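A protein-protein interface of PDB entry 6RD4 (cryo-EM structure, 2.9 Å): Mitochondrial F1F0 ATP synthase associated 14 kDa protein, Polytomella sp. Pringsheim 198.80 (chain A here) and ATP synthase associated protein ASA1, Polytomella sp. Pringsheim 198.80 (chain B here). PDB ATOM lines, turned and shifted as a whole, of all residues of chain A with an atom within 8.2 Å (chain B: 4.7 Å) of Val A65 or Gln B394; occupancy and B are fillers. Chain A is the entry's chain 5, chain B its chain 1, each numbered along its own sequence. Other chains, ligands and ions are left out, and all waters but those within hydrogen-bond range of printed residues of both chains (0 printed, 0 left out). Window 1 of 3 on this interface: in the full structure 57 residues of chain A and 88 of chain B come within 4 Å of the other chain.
The backbone carbonyl oxygen (O) of Leu A68 lies within hydrogen-bond range of the guanidinium group (NH2) of Arg B118 (3.3 Å). The backbone carbonyl oxygen of Leu A66 is in hydrogen-bond range of the guanidinium group of Arg B118, 2.9 Å away.
O of Tyr A62 touches CE2 of Phe B111, 3.7 Å away. Phe B111 touches Asp A63. CG2 of Val A65 touches OE1 of Gln B394, 3.5 Å away. CD2 of Leu A66 touches CD1 of Phe B111 (3.7 Å). Ala A70 touches Ile B115 (CB to O, 3.4 Å). Arg B118 touches Ala A70. CB of Glu B397 touches OG of Ser A72, at 3.4 Å.
Printed residues of chain B within 4 Å of Val A65: Gln B394. Of chain A, only Val A65 comes within 4 Å of Gln B394. Printed residues of chain B within 4 Å of Leu A66: Phe B111 (3.7 Å) and Arg B118 (2.9 Å). Printed residues of chain A within 4 Å of Glu B397: Ser A72 (3.4 Å). Of the printed residues of chain A, Phe B111 touches Tyr A62 (3.7 Å), Asp A63 (3.7 Å) and Leu A66 (3.7 Å). Of the printed residues of chain B, Leu A68 touches Arg B118. Printed residues of chain A within 4 Å of Ile B115: Ala A70. The nearest printed residue of chain B that does not touch Val A65 is Ile B115 (4.0001 Å).
Printed residues of chain B that touch a printed residue of chain A: Phe B111, Ile B115, Arg B118, Gln B394 and Glu B397.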
ATOM      1  N   PRO A  60       0.215   7.182 -15.238  1.00  0.00           N
ATOM      2  CA  PRO A  60       1.132   7.477 -14.141  1.00  0.00           C
ATOM      3  C   PRO A  60       0.425   8.090 -12.960  1.00  0.00           C
ATOM      4  O   PRO A  60       1.046   8.613 -12.041  1.00  0.00           O
ATOM      5  CB  PRO A  60       2.106   8.449 -14.789  1.00  0.00           C
ATOM      6  CG  PRO A  60       1.281   9.154 -15.767  1.00  0.00           C
ATOM      7  CD  PRO A  60       0.162   8.293 -16.197  1.00  0.00           C
ATOM      8  N   SER A  61      -0.884   7.989 -12.979  1.00  0.00           N
ATOM      9  CA  SER A  61      -1.779   8.740 -12.133  1.00  0.00           C
ATOM     10  C   SER A  61      -1.888   8.237 -10.712  1.00  0.00           C
ATOM     11  O   SER A  61      -2.671   8.800  -9.954  1.00  0.00           O
ATOM     12  CB  SER A  61      -3.157   8.716 -12.746  1.00  0.00           C
ATOM     13  OG  SER A  61      -4.083   9.116 -11.785  1.00  0.00           O
ATOM     14  N   TYR A  62      -1.159   7.211 -10.314  1.00  0.00           N
ATOM     15  CA  TYR A  62      -1.355   6.673  -8.976  1.00  0.00           C
ATOM     16  C   TYR A  62      -0.292   7.107  -7.996  1.00  0.00           C
ATOM     17  O   TYR A  62      -0.600   7.387  -6.840  1.00  0.00           O
ATOM     18  CB  TYR A  62      -1.372   5.156  -9.010  1.00  0.00           C
ATOM     19  CG  TYR A  62      -2.359   4.595  -9.960  1.00  0.00           C
ATOM     20  CD1 TYR A  62      -3.702   4.726  -9.728  1.00  0.00           C
ATOM     21  CD2 TYR A  62      -1.948   3.906 -11.066  1.00  0.00           C
ATOM     22  CE1 TYR A  62      -4.600   4.210 -10.581  1.00  0.00           C
ATOM     23  CE2 TYR A  62      -2.841   3.390 -11.922  1.00  0.00           C
ATOM     24  CZ  TYR A  62      -4.165   3.553 -11.677  1.00  0.00           C
ATOM     25  OH  TYR A  62      -5.075   3.028 -12.534  1.00  0.00           O
ATOM     26  N   ASP A  63       0.956   7.129  -8.433  1.00  0.00           N
ATOM     27  CA  ASP A  63       2.086   7.502  -7.602  1.00  0.00           C
ATOM     28  C   ASP A  63       2.564   8.895  -7.931  1.00  0.00           C
ATOM     29  O   ASP A  63       3.760   9.131  -8.076  1.00  0.00           O
ATOM     30  CB  ASP A  63       3.201   6.486  -7.762  1.00  0.00           C
ATOM     31  CG  ASP A  63       3.454   6.129  -9.199  1.00  0.00           C
ATOM     32  OD1 ASP A  63       2.706   6.609 -10.068  1.00  0.00           O
ATOM     33  OD2 ASP A  63       4.399   5.359  -9.468  1.00  0.00           O
ATOM     34  N   ARG A  64       1.630   9.822  -8.120  1.00  0.00           N
ATOM     35  CA  ARG A  64       1.992  11.212  -8.313  1.00  0.00           C
ATOM     36  C   ARG A  64       2.543  11.834  -7.052  1.00  0.00           C
ATOM     37  O   ARG A  64       3.294  12.805  -7.134  1.00  0.00           O
ATOM     38  CB  ARG A  64       0.790  12.019  -8.766  1.00  0.00           C
ATOM     39  CG  ARG A  64       0.258  11.658 -10.100  1.00  0.00           C
ATOM     40  CD  ARG A  64       1.081  12.231 -11.214  1.00  0.00           C
ATOM     41  NE  ARG A  64       0.260  12.313 -12.406  1.00  0.00           N
ATOM     42  CZ  ARG A  64       0.725  12.300 -13.644  1.00  0.00           C
ATOM     43  NH1 ARG A  64       2.020  12.204 -13.871  1.00  0.00           N
ATOM     44  NH2 ARG A  64      -0.114  12.370 -14.653  1.00  0.00           N
ATOM     45  N   VAL A  65       2.188  11.285  -5.889  1.00  0.00           N
ATOM     46  CA  VAL A  65       2.661  11.813  -4.625  1.00  0.00           C
ATOM     47  C   VAL A  65       4.148  11.565  -4.447  1.00  0.00           C
ATOM     48  O   VAL A  65       4.806  12.291  -3.702  1.00  0.00           O
ATOM     49  CB  VAL A  65       1.820  11.207  -3.488  1.00  0.00           C
ATOM     50  CG1 VAL A  65       2.187   9.779  -3.233  1.00  0.00           C
ATOM     51  CG2 VAL A  65       1.929  12.026  -2.237  1.00  0.00           C
ATOM     52  N   LEU A  66       4.717  10.602  -5.153  1.00  0.00           N
ATOM     53  CA  LEU A  66       6.140  10.359  -5.062  1.00  0.00           C
ATOM     54  C   LEU A  66       6.943  11.294  -5.933  1.00  0.00           C
ATOM     55  O   LEU A  66       8.167  11.199  -5.943  1.00  0.00           O
ATOM     56  CB  LEU A  66       6.453   8.919  -5.439  1.00  0.00           C
ATOM     57  CG  LEU A  66       5.746   7.801  -4.700  1.00  0.00           C
ATOM     58  CD1 LEU A  66       6.432   6.522  -5.013  1.00  0.00           C
ATOM     59  CD2 LEU A  66       5.770   8.032  -3.239  1.00  0.00           C
ATOM     60  N   SER A  67       6.301  12.175  -6.681  1.00  0.00           N
ATOM     61  CA  SER A  67       7.003  13.224  -7.395  1.00  0.00           C
ATOM     62  C   SER A  67       6.928  14.557  -6.683  1.00  0.00           C
ATOM     63  O   SER A  67       7.681  15.468  -7.029  1.00  0.00           O
ATOM     64  CB  SER A  67       6.449  13.374  -8.809  1.00  0.00           C
ATOM     65  OG  SER A  67       6.553  12.160  -9.523  1.00  0.00           O
ATOM     66  N   LEU A  68       6.041  14.690  -5.709  1.00  0.00           N
ATOM     67  CA  LEU A  68       6.016  15.851  -4.852  1.00  0.00           C
ATOM     68  C   LEU A  68       7.247  15.848  -3.954  1.00  0.00           C
ATOM     69  O   LEU A  68       7.840  14.795  -3.718  1.00  0.00           O
ATOM     70  CB  LEU A  68       4.755  15.837  -4.006  1.00  0.00           C
ATOM     71  CG  LEU A  68       3.444  16.035  -4.733  1.00  0.00           C
ATOM     72  CD1 LEU A  68       2.359  16.170  -3.719  1.00  0.00           C
ATOM     73  CD2 LEU A  68       3.489  17.235  -5.621  1.00  0.00           C
ATOM     74  N   PRO A  69       7.662  17.010  -3.447  1.00  0.00           N
ATOM     75  CA  PRO A  69       8.790  17.039  -2.514  1.00  0.00           C
ATOM     76  C   PRO A  69       8.432  16.365  -1.200  1.00  0.00           C
ATOM     77  O   PRO A  69       7.440  16.715  -0.563  1.00  0.00           O
ATOM     78  CB  PRO A  69       9.053  18.530  -2.336  1.00  0.00           C
ATOM     79  CG  PRO A  69       7.820  19.175  -2.745  1.00  0.00           C
ATOM     80  CD  PRO A  69       7.277  18.374  -3.838  1.00  0.00           C
ATOM     81  N   ALA A  70       9.247  15.377  -0.818  1.00  0.00           N
ATOM     82  CA  ALA A  70       8.907  14.499   0.294  1.00  0.00           C
ATOM     83  C   ALA A  70       8.998  15.212   1.618  1.00  0.00           C
ATOM     84  O   ALA A  70       8.303  14.842   2.567  1.00  0.00           O
ATOM     85  CB  ALA A  70       9.819  13.283   0.316  1.00  0.00           C
ATOM     86  N   VAL A  71       9.854  16.223   1.701  1.00  0.00           N
ATOM     87  CA  VAL A  71       9.963  17.024   2.907  1.00  0.00           C
ATOM     88  C   VAL A  71       8.722  17.887   3.010  1.00  0.00           C
ATOM     89  O   VAL A  71       8.390  18.628   2.083  1.00  0.00           O
ATOM     90  CB  VAL A  71      11.232  17.873   2.884  1.00  0.00           C
ATOM     91  CG1 VAL A  71      11.447  18.476   4.223  1.00  0.00           C
ATOM     92  CG2 VAL A  71      12.406  17.035   2.518  1.00  0.00           C
ATOM     93  N   SER A  72       8.045  17.803   4.142  1.00  0.00           N
ATOM     94  CA  SER A  72       6.756  18.429   4.330  1.00  0.00           C
ATOM     95  C   SER A  72       6.859  19.942   4.373  1.00  0.00           C
ATOM     96  O   SER A  72       7.942  20.515   4.417  1.00  0.00           O
ATOM     97  CB  SER A  72       6.135  17.943   5.621  1.00  0.00           C
ATOM     98  OG  SER A  72       4.864  18.514   5.783  1.00  0.00           O
ATOM     99  N   PHE B 111       3.665   4.254   0.119  1.00  0.00           N
ATOM    100  CA  PHE B 111       3.935   5.625  -0.285  1.00  0.00           C
ATOM    101  C   PHE B 111       4.492   6.431   0.868  1.00  0.00           C
ATOM    102  O   PHE B 111       5.275   7.355   0.659  1.00  0.00           O
ATOM    103  CB  PHE B 111       2.659   6.284  -0.800  1.00  0.00           C
ATOM    104  CG  PHE B 111       2.267   5.870  -2.175  1.00  0.00           C
ATOM    105  CD1 PHE B 111       3.198   5.386  -3.064  1.00  0.00           C
ATOM    106  CD2 PHE B 111       0.959   5.980  -2.582  1.00  0.00           C
ATOM    107  CE1 PHE B 111       2.828   5.011  -4.319  1.00  0.00           C
ATOM    108  CE2 PHE B 111       0.594   5.606  -3.838  1.00  0.00           C
ATOM    109  CZ  PHE B 111       1.532   5.123  -4.700  1.00  0.00           C
ATOM    110  N   ILE B 115       8.287   8.248   0.960  1.00  0.00           N
ATOM    111  CA  ILE B 115       8.369   9.670   1.246  1.00  0.00           C
ATOM    112  C   ILE B 115       9.224   9.913   2.475  1.00  0.00           C
ATOM    113  O   ILE B 115      10.172  10.701   2.439  1.00  0.00           O
ATOM    114  CB  ILE B 115       6.959  10.249   1.412  1.00  0.00           C
ATOM    115  CG1 ILE B 115       6.307  10.401   0.053  1.00  0.00           C
ATOM    116  CG2 ILE B 115       7.009  11.574   2.057  1.00  0.00           C
ATOM    117  CD1 ILE B 115       4.858  10.704   0.145  1.00  0.00           C
ATOM    118  N   ARG B 118      12.828   9.380   1.855  1.00  0.00           N
ATOM    119  CA  ARG B 118      13.410  10.434   1.046  1.00  0.00           C
ATOM    120  C   ARG B 118      13.401  11.773   1.759  1.00  0.00           C
ATOM    121  O   ARG B 118      14.180  12.654   1.399  1.00  0.00           O
ATOM    122  CB  ARG B 118      12.652  10.517  -0.273  1.00  0.00           C
ATOM    123  CG  ARG B 118      13.418  11.135  -1.408  1.00  0.00           C
ATOM    124  CD  ARG B 118      12.537  11.296  -2.627  1.00  0.00           C
ATOM    125  NE  ARG B 118      11.132  11.437  -2.262  1.00  0.00           N
ATOM    126  CZ  ARG B 118      10.163  11.764  -3.109  1.00  0.00           C
ATOM    127  NH1 ARG B 118      10.449  12.032  -4.373  1.00  0.00           N
ATOM    128  NH2 ARG B 118       8.915  11.849  -2.687  1.00  0.00           N
ATOM    129  N   THR B 384      -6.837  18.666   5.249  1.00  0.00           N
ATOM    130  CA  THR B 384      -6.054  17.474   5.547  1.00  0.00           C
ATOM    131  C   THR B 384      -6.936  16.328   6.002  1.00  0.00           C
ATOM    132  O   THR B 384      -6.644  15.168   5.719  1.00  0.00           O
ATOM    133  CB  THR B 384      -5.008  17.804   6.596  1.00  0.00           C
ATOM    134  OG1 THR B 384      -4.379  19.031   6.233  1.00  0.00           O
ATOM    135  CG2 THR B 384      -3.979  16.765   6.661  1.00  0.00           C
ATOM    136  N   TYR B 388      -6.741  13.079   3.228  1.00  0.00           N
ATOM    137  CA  TYR B 388      -6.020  11.944   3.773  1.00  0.00           C
ATOM    138  C   TYR B 388      -6.807  11.331   4.910  1.00  0.00           C
ATOM    139  O   TYR B 388      -7.610  11.995   5.560  1.00  0.00           O
ATOM    140  CB  TYR B 388      -4.652  12.328   4.293  1.00  0.00           C
ATOM    141  CG  TYR B 388      -3.895  13.257   3.409  1.00  0.00           C
ATOM    142  CD1 TYR B 388      -3.216  12.789   2.314  1.00  0.00           C
ATOM    143  CD2 TYR B 388      -3.864  14.605   3.670  1.00  0.00           C
ATOM    144  CE1 TYR B 388      -2.529  13.636   1.509  1.00  0.00           C
ATOM    145  CE2 TYR B 388      -3.174  15.457   2.872  1.00  0.00           C
ATOM    146  CZ  TYR B 388      -2.512  14.969   1.793  1.00  0.00           C
ATOM    147  OH  TYR B 388      -1.824  15.831   0.988  1.00  0.00           O
ATOM    148  N   ARG B 392      -2.322   8.087   7.380  1.00  0.00           N
ATOM    149  CA  ARG B 392      -1.314   8.528   6.436  1.00  0.00           C
ATOM    150  C   ARG B 392      -0.233   9.353   7.105  1.00  0.00           C
ATOM    151  O   ARG B 392      -0.396   9.865   8.204  1.00  0.00           O
ATOM    152  CB  ARG B 392      -1.951   9.339   5.320  1.00  0.00           C
ATOM    153  CG  ARG B 392      -3.035   8.613   4.610  1.00  0.00           C
ATOM    154  CD  ARG B 392      -2.518   7.383   3.935  1.00  0.00           C
ATOM    155  NE  ARG B 392      -1.457   7.678   2.988  1.00  0.00           N
ATOM    156  CZ  ARG B 392      -1.665   8.053   1.735  1.00  0.00           C
ATOM    157  NH1 ARG B 392      -2.894   8.198   1.284  1.00  0.00           N
ATOM    158  NH2 ARG B 392      -0.645   8.300   0.937  1.00  0.00           N
ATOM    159  N   LEU B 393       0.895   9.452   6.419  1.00  0.00           N
ATOM    160  CA  LEU B 393       1.963  10.336   6.848  1.00  0.00           C
ATOM    161  C   LEU B 393       1.565  11.782   6.673  1.00  0.00           C
ATOM    162  O   LEU B 393       1.863  12.622   7.520  1.00  0.00           O
ATOM    163  CB  LEU B 393       3.209  10.068   6.033  1.00  0.00           C
ATOM    164  CG  LEU B 393       4.432  10.868   6.394  1.00  0.00           C
ATOM    165  CD1 LEU B 393       4.938  10.342   7.690  1.00  0.00           C
ATOM    166  CD2 LEU B 393       5.444  10.734   5.321  1.00  0.00           C
ATOM    167  N   GLN B 394       0.908  12.092   5.569  1.00  0.00           N
ATOM    168  CA  GLN B 394       0.600  13.464   5.233  1.00  0.00           C
ATOM    169  C   GLN B 394      -0.605  13.985   5.975  1.00  0.00           C
ATOM    170  O   GLN B 394      -0.862  15.185   5.926  1.00  0.00           O
ATOM    171  CB  GLN B 394       0.392  13.570   3.739  1.00  0.00           C
ATOM    172  CG  GLN B 394       1.524  12.950   2.987  1.00  0.00           C
ATOM    173  CD  GLN B 394       1.417  13.153   1.511  1.00  0.00           C
ATOM    174  OE1 GLN B 394       0.433  12.770   0.894  1.00  0.00           O
ATOM    175  NE2 GLN B 394       2.434  13.763   0.926  1.00  0.00           N
ATOM    176  N   TYR B 395      -1.353  13.121   6.643  1.00  0.00           N
ATOM    177  CA  TYR B 395      -2.308  13.597   7.625  1.00  0.00           C
ATOM    178  C   TYR B 395      -1.584  14.087   8.860  1.00  0.00           C
ATOM    179  O   TYR B 395      -1.949  15.113   9.438  1.00  0.00           O
ATOM    180  CB  TYR B 395      -3.272  12.487   7.986  1.00  0.00           C
ATOM    181  CG  TYR B 395      -4.373  12.861   8.935  1.00  0.00           C
ATOM    182  CD1 TYR B 395      -5.574  13.317   8.464  1.00  0.00           C
ATOM    183  CD2 TYR B 395      -4.226  12.711  10.304  1.00  0.00           C
ATOM    184  CE1 TYR B 395      -6.582  13.637   9.313  1.00  0.00           C
ATOM    185  CE2 TYR B 395      -5.234  13.028  11.161  1.00  0.00           C
ATOM    186  CZ  TYR B 395      -6.411  13.489  10.655  1.00  0.00           C
ATOM    187  OH  TYR B 395      -7.435  13.812  11.500  1.00  0.00           O
ATOM    188  N   LYS B 396      -0.569  13.349   9.290  1.00  0.00           N
ATOM    189  CA  LYS B 396       0.197  13.741  10.458  1.00  0.00           C
ATOM    190  C   LYS B 396       1.028  14.981  10.185  1.00  0.00           C
ATOM    191  O   LYS B 396       1.139  15.849  11.047  1.00  0.00           O
ATOM    192  CB  LYS B 396       1.072  12.583  10.900  1.00  0.00           C
ATOM    193  CG  LYS B 396       0.267  11.378  11.288  1.00  0.00           C
ATOM    194  CD  LYS B 396       1.101  10.130  11.270  1.00  0.00           C
ATOM    195  CE  LYS B 396       0.252   8.933  11.596  1.00  0.00           C
ATOM    196  NZ  LYS B 396       1.018   7.689  11.389  1.00  0.00           N
ATOM    197  N   GLU B 397       1.595  15.104   8.992  1.00  0.00           N
ATOM    198  CA  GLU B 397       2.355  16.299   8.669  1.00  0.00           C
ATOM    199  C   GLU B 397       1.473  17.476   8.328  1.00  0.00           C
ATOM    200  O   GLU B 397       1.986  18.574   8.123  1.00  0.00           O
ATOM    201  CB  GLU B 397       3.295  16.051   7.503  1.00  0.00           C
ATOM    202  CG  GLU B 397       4.340  15.023   7.780  1.00  0.00           C
ATOM    203  CD  GLU B 397       5.306  15.451   8.851  1.00  0.00           C
ATOM    204  OE1 GLU B 397       5.695  16.631   8.875  1.00  0.00           O
ATOM    205  OE2 GLU B 397       5.677  14.598   9.679  1.00  0.00           O
ATOM    206  N   GLY B 398       0.178  17.270   8.200  1.00  0.00           N
ATOM    207  CA  GLY B 398      -0.697  18.353   7.829  1.00  0.00           C
ATOM    208  C   GLY B 398      -1.344  18.943   9.047  1.00  0.00           C
ATOM    209  O   GLY B 398      -1.661  20.125   9.088  1.00  0.00           O
